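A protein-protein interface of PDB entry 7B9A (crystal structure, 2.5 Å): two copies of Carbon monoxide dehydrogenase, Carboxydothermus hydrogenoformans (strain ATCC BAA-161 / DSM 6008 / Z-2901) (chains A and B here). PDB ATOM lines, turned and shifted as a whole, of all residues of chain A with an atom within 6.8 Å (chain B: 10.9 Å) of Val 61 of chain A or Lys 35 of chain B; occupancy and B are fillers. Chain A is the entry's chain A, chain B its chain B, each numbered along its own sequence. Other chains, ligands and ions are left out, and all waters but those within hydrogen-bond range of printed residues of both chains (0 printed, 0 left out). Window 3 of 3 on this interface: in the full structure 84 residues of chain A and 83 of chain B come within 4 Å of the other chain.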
ATOM      1  N   TYR A  40      10.117 -16.008  -6.412  1.00  0.00           N
ATOM      2  CA  TYR A  40       9.471 -15.363  -7.550  1.00  0.00           C
ATOM      3  C   TYR A  40       8.560 -16.339  -8.288  1.00  0.00           C
ATOM      4  O   TYR A  40       7.359 -16.093  -8.445  1.00  0.00           O
ATOM      5  CB  TYR A  40      10.526 -14.796  -8.503  1.00  0.00           C
ATOM      6  CG  TYR A  40      11.281 -13.592  -7.985  1.00  0.00           C
ATOM      7  CD1 TYR A  40      10.717 -12.321  -8.027  1.00  0.00           C
ATOM      8  CD2 TYR A  40      12.569 -13.719  -7.480  1.00  0.00           C
ATOM      9  CE1 TYR A  40      11.408 -11.216  -7.565  1.00  0.00           C
ATOM     10  CE2 TYR A  40      13.266 -12.621  -7.018  1.00  0.00           C
ATOM     11  CZ  TYR A  40      12.682 -11.373  -7.062  1.00  0.00           C
ATOM     12  OH  TYR A  40      13.377 -10.279  -6.603  1.00  0.00           O
ATOM     13  N   ILE A  57       8.967  -9.642 -10.913  1.00  0.00           N
ATOM     14  CA  ILE A  57       8.201  -8.525 -10.375  1.00  0.00           C
ATOM     15  C   ILE A  57       8.762  -8.208  -8.995  1.00  0.00           C
ATOM     16  O   ILE A  57       8.665  -9.022  -8.070  1.00  0.00           O
ATOM     17  CB  ILE A  57       6.702  -8.837 -10.311  1.00  0.00           C
ATOM     18  CG1 ILE A  57       6.156  -9.112 -11.713  1.00  0.00           C
ATOM     19  CG2 ILE A  57       5.949  -7.685  -9.666  1.00  0.00           C
ATOM     20  CD1 ILE A  57       6.230  -7.921 -12.643  1.00  0.00           C
ATOM     21  N   ASN A  58       9.353  -7.022  -8.856  1.00  0.00           N
ATOM     22  CA  ASN A  58       9.924  -6.581  -7.582  1.00  0.00           C
ATOM     23  C   ASN A  58       9.796  -5.057  -7.544  1.00  0.00           C
ATOM     24  O   ASN A  58      10.657  -4.334  -8.050  1.00  0.00           O
ATOM     25  CB  ASN A  58      11.369  -7.036  -7.432  1.00  0.00           C
ATOM     26  CG  ASN A  58      11.880  -6.895  -6.013  1.00  0.00           C
ATOM     27  OD1 ASN A  58      11.305  -6.170  -5.204  1.00  0.00           O
ATOM     28  ND2 ASN A  58      12.968  -7.591  -5.703  1.00  0.00           N
ATOM     29  N   GLU A  59       8.704  -4.583  -6.940  1.00  0.00           N
ATOM     30  CA  GLU A  59       8.424  -3.151  -6.937  1.00  0.00           C
ATOM     31  C   GLU A  59       9.336  -2.394  -5.979  1.00  0.00           C
ATOM     32  O   GLU A  59       9.604  -1.206  -6.195  1.00  0.00           O
ATOM     33  CB  GLU A  59       6.958  -2.906  -6.585  1.00  0.00           C
ATOM     34  CG  GLU A  59       5.982  -3.534  -7.565  1.00  0.00           C
ATOM     35  CD  GLU A  59       4.541  -3.439  -7.102  1.00  0.00           C
ATOM     36  OE1 GLU A  59       4.209  -2.483  -6.371  1.00  0.00           O
ATOM     37  OE2 GLU A  59       3.741  -4.328  -7.466  1.00  0.00           O
ATOM     38  N   LYS A  60       9.822  -3.052  -4.925  1.00  0.00           N
ATOM     39  CA  LYS A  60      10.696  -2.371  -3.977  1.00  0.00           C
ATOM     40  C   LYS A  60      12.087  -2.112  -4.543  1.00  0.00           C
ATOM     41  O   LYS A  60      12.847  -1.346  -3.941  1.00  0.00           O
ATOM     42  CB  LYS A  60      10.799  -3.174  -2.676  1.00  0.00           C
ATOM     43  CG  LYS A  60      11.746  -4.361  -2.726  1.00  0.00           C
ATOM     44  CD  LYS A  60      11.746  -5.119  -1.406  1.00  0.00           C
ATOM     45  CE  LYS A  60      10.428  -5.849  -1.175  1.00  0.00           C
ATOM     46  NZ  LYS A  60      10.390  -7.172  -1.862  1.00  0.00           N
ATOM     47  N   VAL A  61      12.436  -2.720  -5.677  1.00  0.00           N
ATOM     48  CA  VAL A  61      13.690  -2.439  -6.367  1.00  0.00           C
ATOM     49  C   VAL A  61      13.476  -1.688  -7.669  1.00  0.00           C
ATOM     50  O   VAL A  61      14.459  -1.354  -8.348  1.00  0.00           O
ATOM     51  CB  VAL A  61      14.497  -3.728  -6.620  1.00  0.00           C
ATOM     52  CG1 VAL A  61      14.561  -4.576  -5.358  1.00  0.00           C
ATOM     53  CG2 VAL A  61      13.903  -4.515  -7.779  1.00  0.00           C
ATOM     54  N   GLY A  62      12.228  -1.414  -8.046  1.00  0.00           N
ATOM     55  CA  GLY A  62      11.927  -0.629  -9.228  1.00  0.00           C
ATOM     56  C   GLY A  62      11.376  -1.408 -10.403  1.00  0.00           C
ATOM     57  O   GLY A  62      11.081  -0.800 -11.438  1.00  0.00           O
ATOM     58  N   ALA A  63      11.223  -2.725 -10.286  1.00  0.00           N
ATOM     59  CA  ALA A  63      10.723  -3.550 -11.385  1.00  0.00           C
ATOM     60  C   ALA A  63       9.242  -3.858 -11.164  1.00  0.00           C
ATOM     61  O   ALA A  63       8.840  -4.974 -10.837  1.00  0.00           O
ATOM     62  CB  ALA A  63      11.553  -4.824 -11.510  1.00  0.00           C
ATOM     63  N   THR A  64       8.423  -2.821 -11.357  1.00  0.00           N
ATOM     64  CA  THR A  64       6.984  -2.964 -11.155  1.00  0.00           C
ATOM     65  C   THR A  64       6.355  -3.825 -12.244  1.00  0.00           C
ATOM     66  O   THR A  64       5.536  -4.706 -11.953  1.00  0.00           O
ATOM     67  CB  THR A  64       6.322  -1.587 -11.107  1.00  0.00           C
ATOM     68  OG1 THR A  64       6.809  -0.861  -9.971  1.00  0.00           O
ATOM     69  CG2 THR A  64       4.809  -1.720 -11.005  1.00  0.00           C
ATOM     70  N   THR B   3      19.956   2.736 -20.314  1.00  0.00           N
ATOM     71  CA  THR B   3      21.227   2.383 -20.937  1.00  0.00           C
ATOM     72  C   THR B   3      21.069   1.975 -22.396  1.00  0.00           C
ATOM     73  O   THR B   3      22.060   1.971 -23.134  1.00  0.00           O
ATOM     74  CB  THR B   3      21.907   1.255 -20.156  1.00  0.00           C
ATOM     75  OG1 THR B   3      20.950   0.231 -19.854  1.00  0.00           O
ATOM     76  CG2 THR B   3      22.509   1.786 -18.864  1.00  0.00           C
ATOM     77  N   LYS B   4      19.856   1.637 -22.828  1.00  0.00           N
ATOM     78  CA  LYS B   4      19.608   1.230 -24.204  1.00  0.00           C
ATOM     79  C   LYS B   4      18.334   1.888 -24.706  1.00  0.00           C
ATOM     80  O   LYS B   4      17.321   1.911 -24.000  1.00  0.00           O
ATOM     81  CB  LYS B   4      19.502  -0.296 -24.322  1.00  0.00           C
ATOM     82  CG  LYS B   4      20.813  -0.976 -24.690  1.00  0.00           C
ATOM     83  CD  LYS B   4      20.699  -2.489 -24.626  1.00  0.00           C
ATOM     84  CE  LYS B   4      20.939  -2.996 -23.215  1.00  0.00           C
ATOM     85  NZ  LYS B   4      20.814  -4.478 -23.127  1.00  0.00           N
ATOM     86  N   PHE B  27      12.037   0.728 -22.829  1.00  0.00           N
ATOM     87  CA  PHE B  27      13.431   1.117 -22.643  1.00  0.00           C
ATOM     88  C   PHE B  27      13.734   1.386 -21.175  1.00  0.00           C
ATOM     89  O   PHE B  27      14.778   0.967 -20.660  1.00  0.00           O
ATOM     90  CB  PHE B  27      13.755   2.350 -23.489  1.00  0.00           C
ATOM     91  CG  PHE B  27      13.163   2.314 -24.871  1.00  0.00           C
ATOM     92  CD1 PHE B  27      13.733   1.538 -25.867  1.00  0.00           C
ATOM     93  CD2 PHE B  27      12.041   3.069 -25.176  1.00  0.00           C
ATOM     94  CE1 PHE B  27      13.189   1.508 -27.140  1.00  0.00           C
ATOM     95  CE2 PHE B  27      11.493   3.044 -26.447  1.00  0.00           C
ATOM     96  CZ  PHE B  27      12.068   2.263 -27.429  1.00  0.00           C
ATOM     97  N   ASP B  28      12.824   2.071 -20.478  1.00  0.00           N
ATOM     98  CA  ASP B  28      13.033   2.338 -19.059  1.00  0.00           C
ATOM     99  C   ASP B  28      12.797   1.098 -18.207  1.00  0.00           C
ATOM    100  O   ASP B  28      13.451   0.931 -17.173  1.00  0.00           O
ATOM    101  CB  ASP B  28      12.127   3.477 -18.596  1.00  0.00           C
ATOM    102  CG  ASP B  28      12.630   4.838 -19.033  1.00  0.00           C
ATOM    103  OD1 ASP B  28      13.848   4.974 -19.272  1.00  0.00           O
ATOM    104  OD2 ASP B  28      11.808   5.774 -19.132  1.00  0.00           O
ATOM    105  N   ARG B  29      11.876   0.225 -18.614  1.00  0.00           N
ATOM    106  CA  ARG B  29      11.587  -0.979 -17.846  1.00  0.00           C
ATOM    107  C   ARG B  29      12.653  -2.057 -17.997  1.00  0.00           C
ATOM    108  O   ARG B  29      12.660  -3.009 -17.209  1.00  0.00           O
ATOM    109  CB  ARG B  29      10.224  -1.555 -18.247  1.00  0.00           C
ATOM    110  CG  ARG B  29       9.034  -0.711 -17.814  1.00  0.00           C
ATOM    111  CD  ARG B  29       7.718  -1.376 -18.191  1.00  0.00           C
ATOM    112  NE  ARG B  29       7.570  -1.542 -19.635  1.00  0.00           N
ATOM    113  CZ  ARG B  29       6.735  -0.835 -20.391  1.00  0.00           C
ATOM    114  NH1 ARG B  29       5.959   0.088 -19.841  1.00  0.00           N
ATOM    115  NH2 ARG B  29       6.670  -1.057 -21.697  1.00  0.00           N
ATOM    116  N   PHE B  30      13.547  -1.937 -18.981  1.00  0.00           N
ATOM    117  CA  PHE B  30      14.560  -2.969 -19.178  1.00  0.00           C
ATOM    118  C   PHE B  30      15.595  -2.968 -18.056  1.00  0.00           C
ATOM    119  O   PHE B  30      16.034  -4.035 -17.610  1.00  0.00           O
ATOM    120  CB  PHE B  30      15.245  -2.784 -20.533  1.00  0.00           C
ATOM    121  CG  PHE B  30      16.111  -3.945 -20.938  1.00  0.00           C
ATOM    122  CD1 PHE B  30      15.559  -5.050 -21.564  1.00  0.00           C
ATOM    123  CD2 PHE B  30      17.475  -3.931 -20.693  1.00  0.00           C
ATOM    124  CE1 PHE B  30      16.350  -6.120 -21.937  1.00  0.00           C
ATOM    125  CE2 PHE B  30      18.270  -4.999 -21.067  1.00  0.00           C
ATOM    126  CZ  PHE B  30      17.707  -6.095 -21.690  1.00  0.00           C
ATOM    127  N   ASP B  31      15.996  -1.782 -17.583  1.00  0.00           N
ATOM    128  CA  ASP B  31      17.105  -1.715 -16.632  1.00  0.00           C
ATOM    129  C   ASP B  31      16.751  -2.279 -15.258  1.00  0.00           C
ATOM    130  O   ASP B  31      17.560  -3.047 -14.709  1.00  0.00           O
ATOM    131  CB  ASP B  31      17.623  -0.277 -16.538  1.00  0.00           C
ATOM    132  CG  ASP B  31      18.103   0.255 -17.872  1.00  0.00           C
ATOM    133  OD1 ASP B  31      18.508  -0.559 -18.730  1.00  0.00           O
ATOM    134  OD2 ASP B  31      18.075   1.488 -18.064  1.00  0.00           O
ATOM    135  N   PRO B  32      15.609  -1.947 -14.640  1.00  0.00           N
ATOM    136  CA  PRO B  32      15.298  -2.563 -13.338  1.00  0.00           C
ATOM    137  C   PRO B  32      15.247  -4.080 -13.387  1.00  0.00           C
ATOM    138  O   PRO B  32      15.546  -4.734 -12.379  1.00  0.00           O
ATOM    139  CB  PRO B  32      13.931  -1.961 -12.984  1.00  0.00           C
ATOM    140  CG  PRO B  32      13.905  -0.659 -13.700  1.00  0.00           C
ATOM    141  CD  PRO B  32      14.620  -0.911 -14.993  1.00  0.00           C
ATOM    142  N   GLN B  33      14.880  -4.662 -14.531  1.00  0.00           N
ATOM    143  CA  GLN B  33      14.945  -6.108 -14.687  1.00  0.00           C
ATOM    144  C   GLN B  33      16.381  -6.610 -14.783  1.00  0.00           C
ATOM    145  O   GLN B  33      16.642  -7.769 -14.445  1.00  0.00           O
ATOM    146  CB  GLN B  33      14.161  -6.541 -15.928  1.00  0.00           C
ATOM    147  CG  GLN B  33      12.661  -6.301 -15.837  1.00  0.00           C
ATOM    148  CD  GLN B  33      11.985  -7.209 -14.828  1.00  0.00           C
ATOM    149  OE1 GLN B  33      12.545  -8.228 -14.418  1.00  0.00           O
ATOM    150  NE2 GLN B  33      10.775  -6.845 -14.421  1.00  0.00           N
ATOM    151  N   GLU B  34      17.316  -5.764 -15.226  1.00  0.00           N
ATOM    152  CA  GLU B  34      18.711  -6.176 -15.343  1.00  0.00           C
ATOM    153  C   GLU B  34      19.404  -6.310 -13.994  1.00  0.00           C
ATOM    154  O   GLU B  34      20.399  -7.032 -13.894  1.00  0.00           O
ATOM    155  CB  GLU B  34      19.473  -5.184 -16.218  1.00  0.00           C
ATOM    156  CG  GLU B  34      19.368  -5.472 -17.703  1.00  0.00           C
ATOM    157  CD  GLU B  34      20.103  -6.736 -18.091  1.00  0.00           C
ATOM    158  OE1 GLU B  34      21.299  -6.857 -17.747  1.00  0.00           O
ATOM    159  OE2 GLU B  34      19.485  -7.613 -18.731  1.00  0.00           O
ATOM    160  N   LYS B  35      18.910  -5.630 -12.958  1.00  0.00           N
ATOM    161  CA  LYS B  35      19.550  -5.728 -11.650  1.00  0.00           C
ATOM    162  C   LYS B  35      19.299  -7.082 -11.005  1.00  0.00           C
ATOM    163  O   LYS B  35      20.099  -7.532 -10.177  1.00  0.00           O
ATOM    164  CB  LYS B  35      19.049  -4.606 -10.739  1.00  0.00           C
ATOM    165  CG  LYS B  35      18.643  -3.346 -11.483  1.00  0.00           C
ATOM    166  CD  LYS B  35      17.836  -2.387 -10.610  1.00  0.00           C
ATOM    167  CE  LYS B  35      18.723  -1.588  -9.669  1.00  0.00           C
ATOM    168  NZ  LYS B  35      17.980  -0.435  -9.085  1.00  0.00           N
ATOM    169  N   ILE B  36      18.201  -7.742 -11.372  1.00  0.00           N
ATOM    170  CA  ILE B  36      17.745  -8.940 -10.675  1.00  0.00           C
ATOM    171  C   ILE B  36      17.490 -10.081 -11.657  1.00  0.00           C
ATOM    172  O   ILE B  36      16.593 -10.906 -11.443  1.00  0.00           O
ATOM    173  CB  ILE B  36      16.476  -8.639  -9.854  1.00  0.00           C
ATOM    174  CG1 ILE B  36      15.368  -8.099 -10.766  1.00  0.00           C
ATOM    175  CG2 ILE B  36      16.789  -7.651  -8.734  1.00  0.00           C
ATOM    176  CD1 ILE B  36      14.029  -7.943 -10.077  1.00  0.00           C
ATOM    177  N   ARG B  37      18.278 -10.145 -12.729  1.00  0.00           N
ATOM    178  CA  ARG B  37      18.104 -11.202 -13.718  1.00  0.00           C
ATOM    179  C   ARG B  37      18.360 -12.575 -13.110  1.00  0.00           C
ATOM    180  O   ARG B  37      19.335 -12.780 -12.384  1.00  0.00           O
ATOM    181  CB  ARG B  37      19.037 -10.986 -14.908  1.00  0.00           C
ATOM    182  CG  ARG B  37      18.661  -9.821 -15.807  1.00  0.00           C
ATOM    183  CD  ARG B  37      17.346 -10.071 -16.537  1.00  0.00           C
ATOM    184  NE  ARG B  37      17.096  -9.052 -17.554  1.00  0.00           N
ATOM    185  CZ  ARG B  37      15.940  -8.898 -18.192  1.00  0.00           C
ATOM    186  NH1 ARG B  37      15.806  -7.944 -19.104  1.00  0.00           N
ATOM    187  NH2 ARG B  37      14.914  -9.693 -17.914  1.00  0.00           N
ATOM    188  N   CYS B  38      17.475 -13.517 -13.418  1.00  0.00           N
ATOM    189  CA  CYS B  38      17.636 -14.896 -12.981  1.00  0.00           C
ATOM    190  C   CYS B  38      18.530 -15.621 -13.975  1.00  0.00           C
ATOM    191  O   CYS B  38      18.152 -15.805 -15.138  1.00  0.00           O
ATOM    192  CB  CYS B  38      16.277 -15.579 -12.866  1.00  0.00           C
ATOM    193  SG  CYS B  38      16.346 -17.314 -12.403  1.00  0.00           S
ATOM    194  N   ASN B  39      19.710 -16.039 -13.515  1.00  0.00           N
ATOM    195  CA  ASN B  39      20.618 -16.775 -14.388  1.00  0.00           C
ATOM    196  C   ASN B  39      20.057 -18.142 -14.749  1.00  0.00           C
ATOM    197  O   ASN B  39      20.330 -18.656 -15.841  1.00  0.00           O
ATOM    198  CB  ASN B  39      21.985 -16.925 -13.724  1.00  0.00           C
ATOM    199  CG  ASN B  39      23.093 -17.207 -14.725  1.00  0.00           C
ATOM    200  OD1 ASN B  39      23.226 -16.519 -15.734  1.00  0.00           O
ATOM    201  ND2 ASN B  39      23.891 -18.236 -14.449  1.00  0.00           N
ATOM    202  N   LYS B 453      17.301  -6.988 -25.822  1.00  0.00           N
ATOM    203  CA  LYS B 453      18.145  -7.905 -25.063  1.00  0.00           C
ATOM    204  C   LYS B 453      19.615  -7.750 -25.436  1.00  0.00           C
ATOM    205  O   LYS B 453      20.464  -7.498 -24.574  1.00  0.00           O
ATOM    206  CB  LYS B 453      17.680  -9.344 -25.285  1.00  0.00           C
ATOM    207  CG  LYS B 453      18.398 -10.363 -24.422  1.00  0.00           C
ATOM    208  CD  LYS B 453      18.235 -10.044 -22.945  1.00  0.00           C
ATOM    209  CE  LYS B 453      18.781 -11.167 -22.081  1.00  0.00           C
ATOM    210  NZ  LYS B 453      18.114 -12.462 -22.387  1.00  0.00           N
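CD1 of Ile 36 of chain B touches CB of Asn 58 of chain A (3.9 Å).
Lys 35 of chain B touches Val 61 of chain A (NZ to O, 3.7 Å).
Gly 62 of chain A touches Pro 32 of chain B (O to CB, 3.4 Å).
Pro 32 of chain B touches Ala 63 of chain A.
Ala 63 of chain A touches Gln 33 of chain B (CB to NE2, 3.6 Å).
OD1 of Asn 58 of chain A sits close to N of Lys 60 of chain A, at 3.5 Å.
The backbone carbonyl oxygen (O) of Gln 33 of chain B lies close to the guanidinium group (NE) of Arg 37 of chain B, at 3.4 Å.
OH of Tyr 40 of chain A lies within hydrogen-bond range of ND2 of Asn 58 of chain A (2.9 Å).
The backbone carbonyl oxygen of Asn 58 of chain A is in hydrogen-bond range of the backbone NH of Ala 63 of chain A, at 2.8 Å.
No position is printed for both chains.
Of the 16 printed residues of chain B, 4 touch a printed residue of chain A.
Printed residues of chain B that touch a printed residue of chain A: Pro 32, Gln 33, Lys 35 and Ile 36.
Hydrophobic or aromatic side chains of chain B that line the printed part of chain A: Pro 32 and Ile 36.
Hydrophobic or aromatic side chains of chain A that line the printed part of chain B: Ala 63.
Among the printed residues, no Asp or Glu carboxylate lies within 4 Å of a Lys or Arg side-chain nitrogen of the other chain.
Of chain B, only Lys 35 (3.7 Å) comes within 4 Å of Val 61 of chain A.
Ala 63 of chain A touches two residues of chain B.
Phe 27 of chain B touches none of the printed residues of chain A.
Printed residues of chain A within 4 Å of Pro 32 of chain B: Gly 62 and Ala 63.
Lys 35 of chain B touches just one residue of chain A: Val 61 (3.7 Å).
Printed residues of chain A within 4 Å of Ile 36 of chain B: Asn 58 (3.9 Å).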
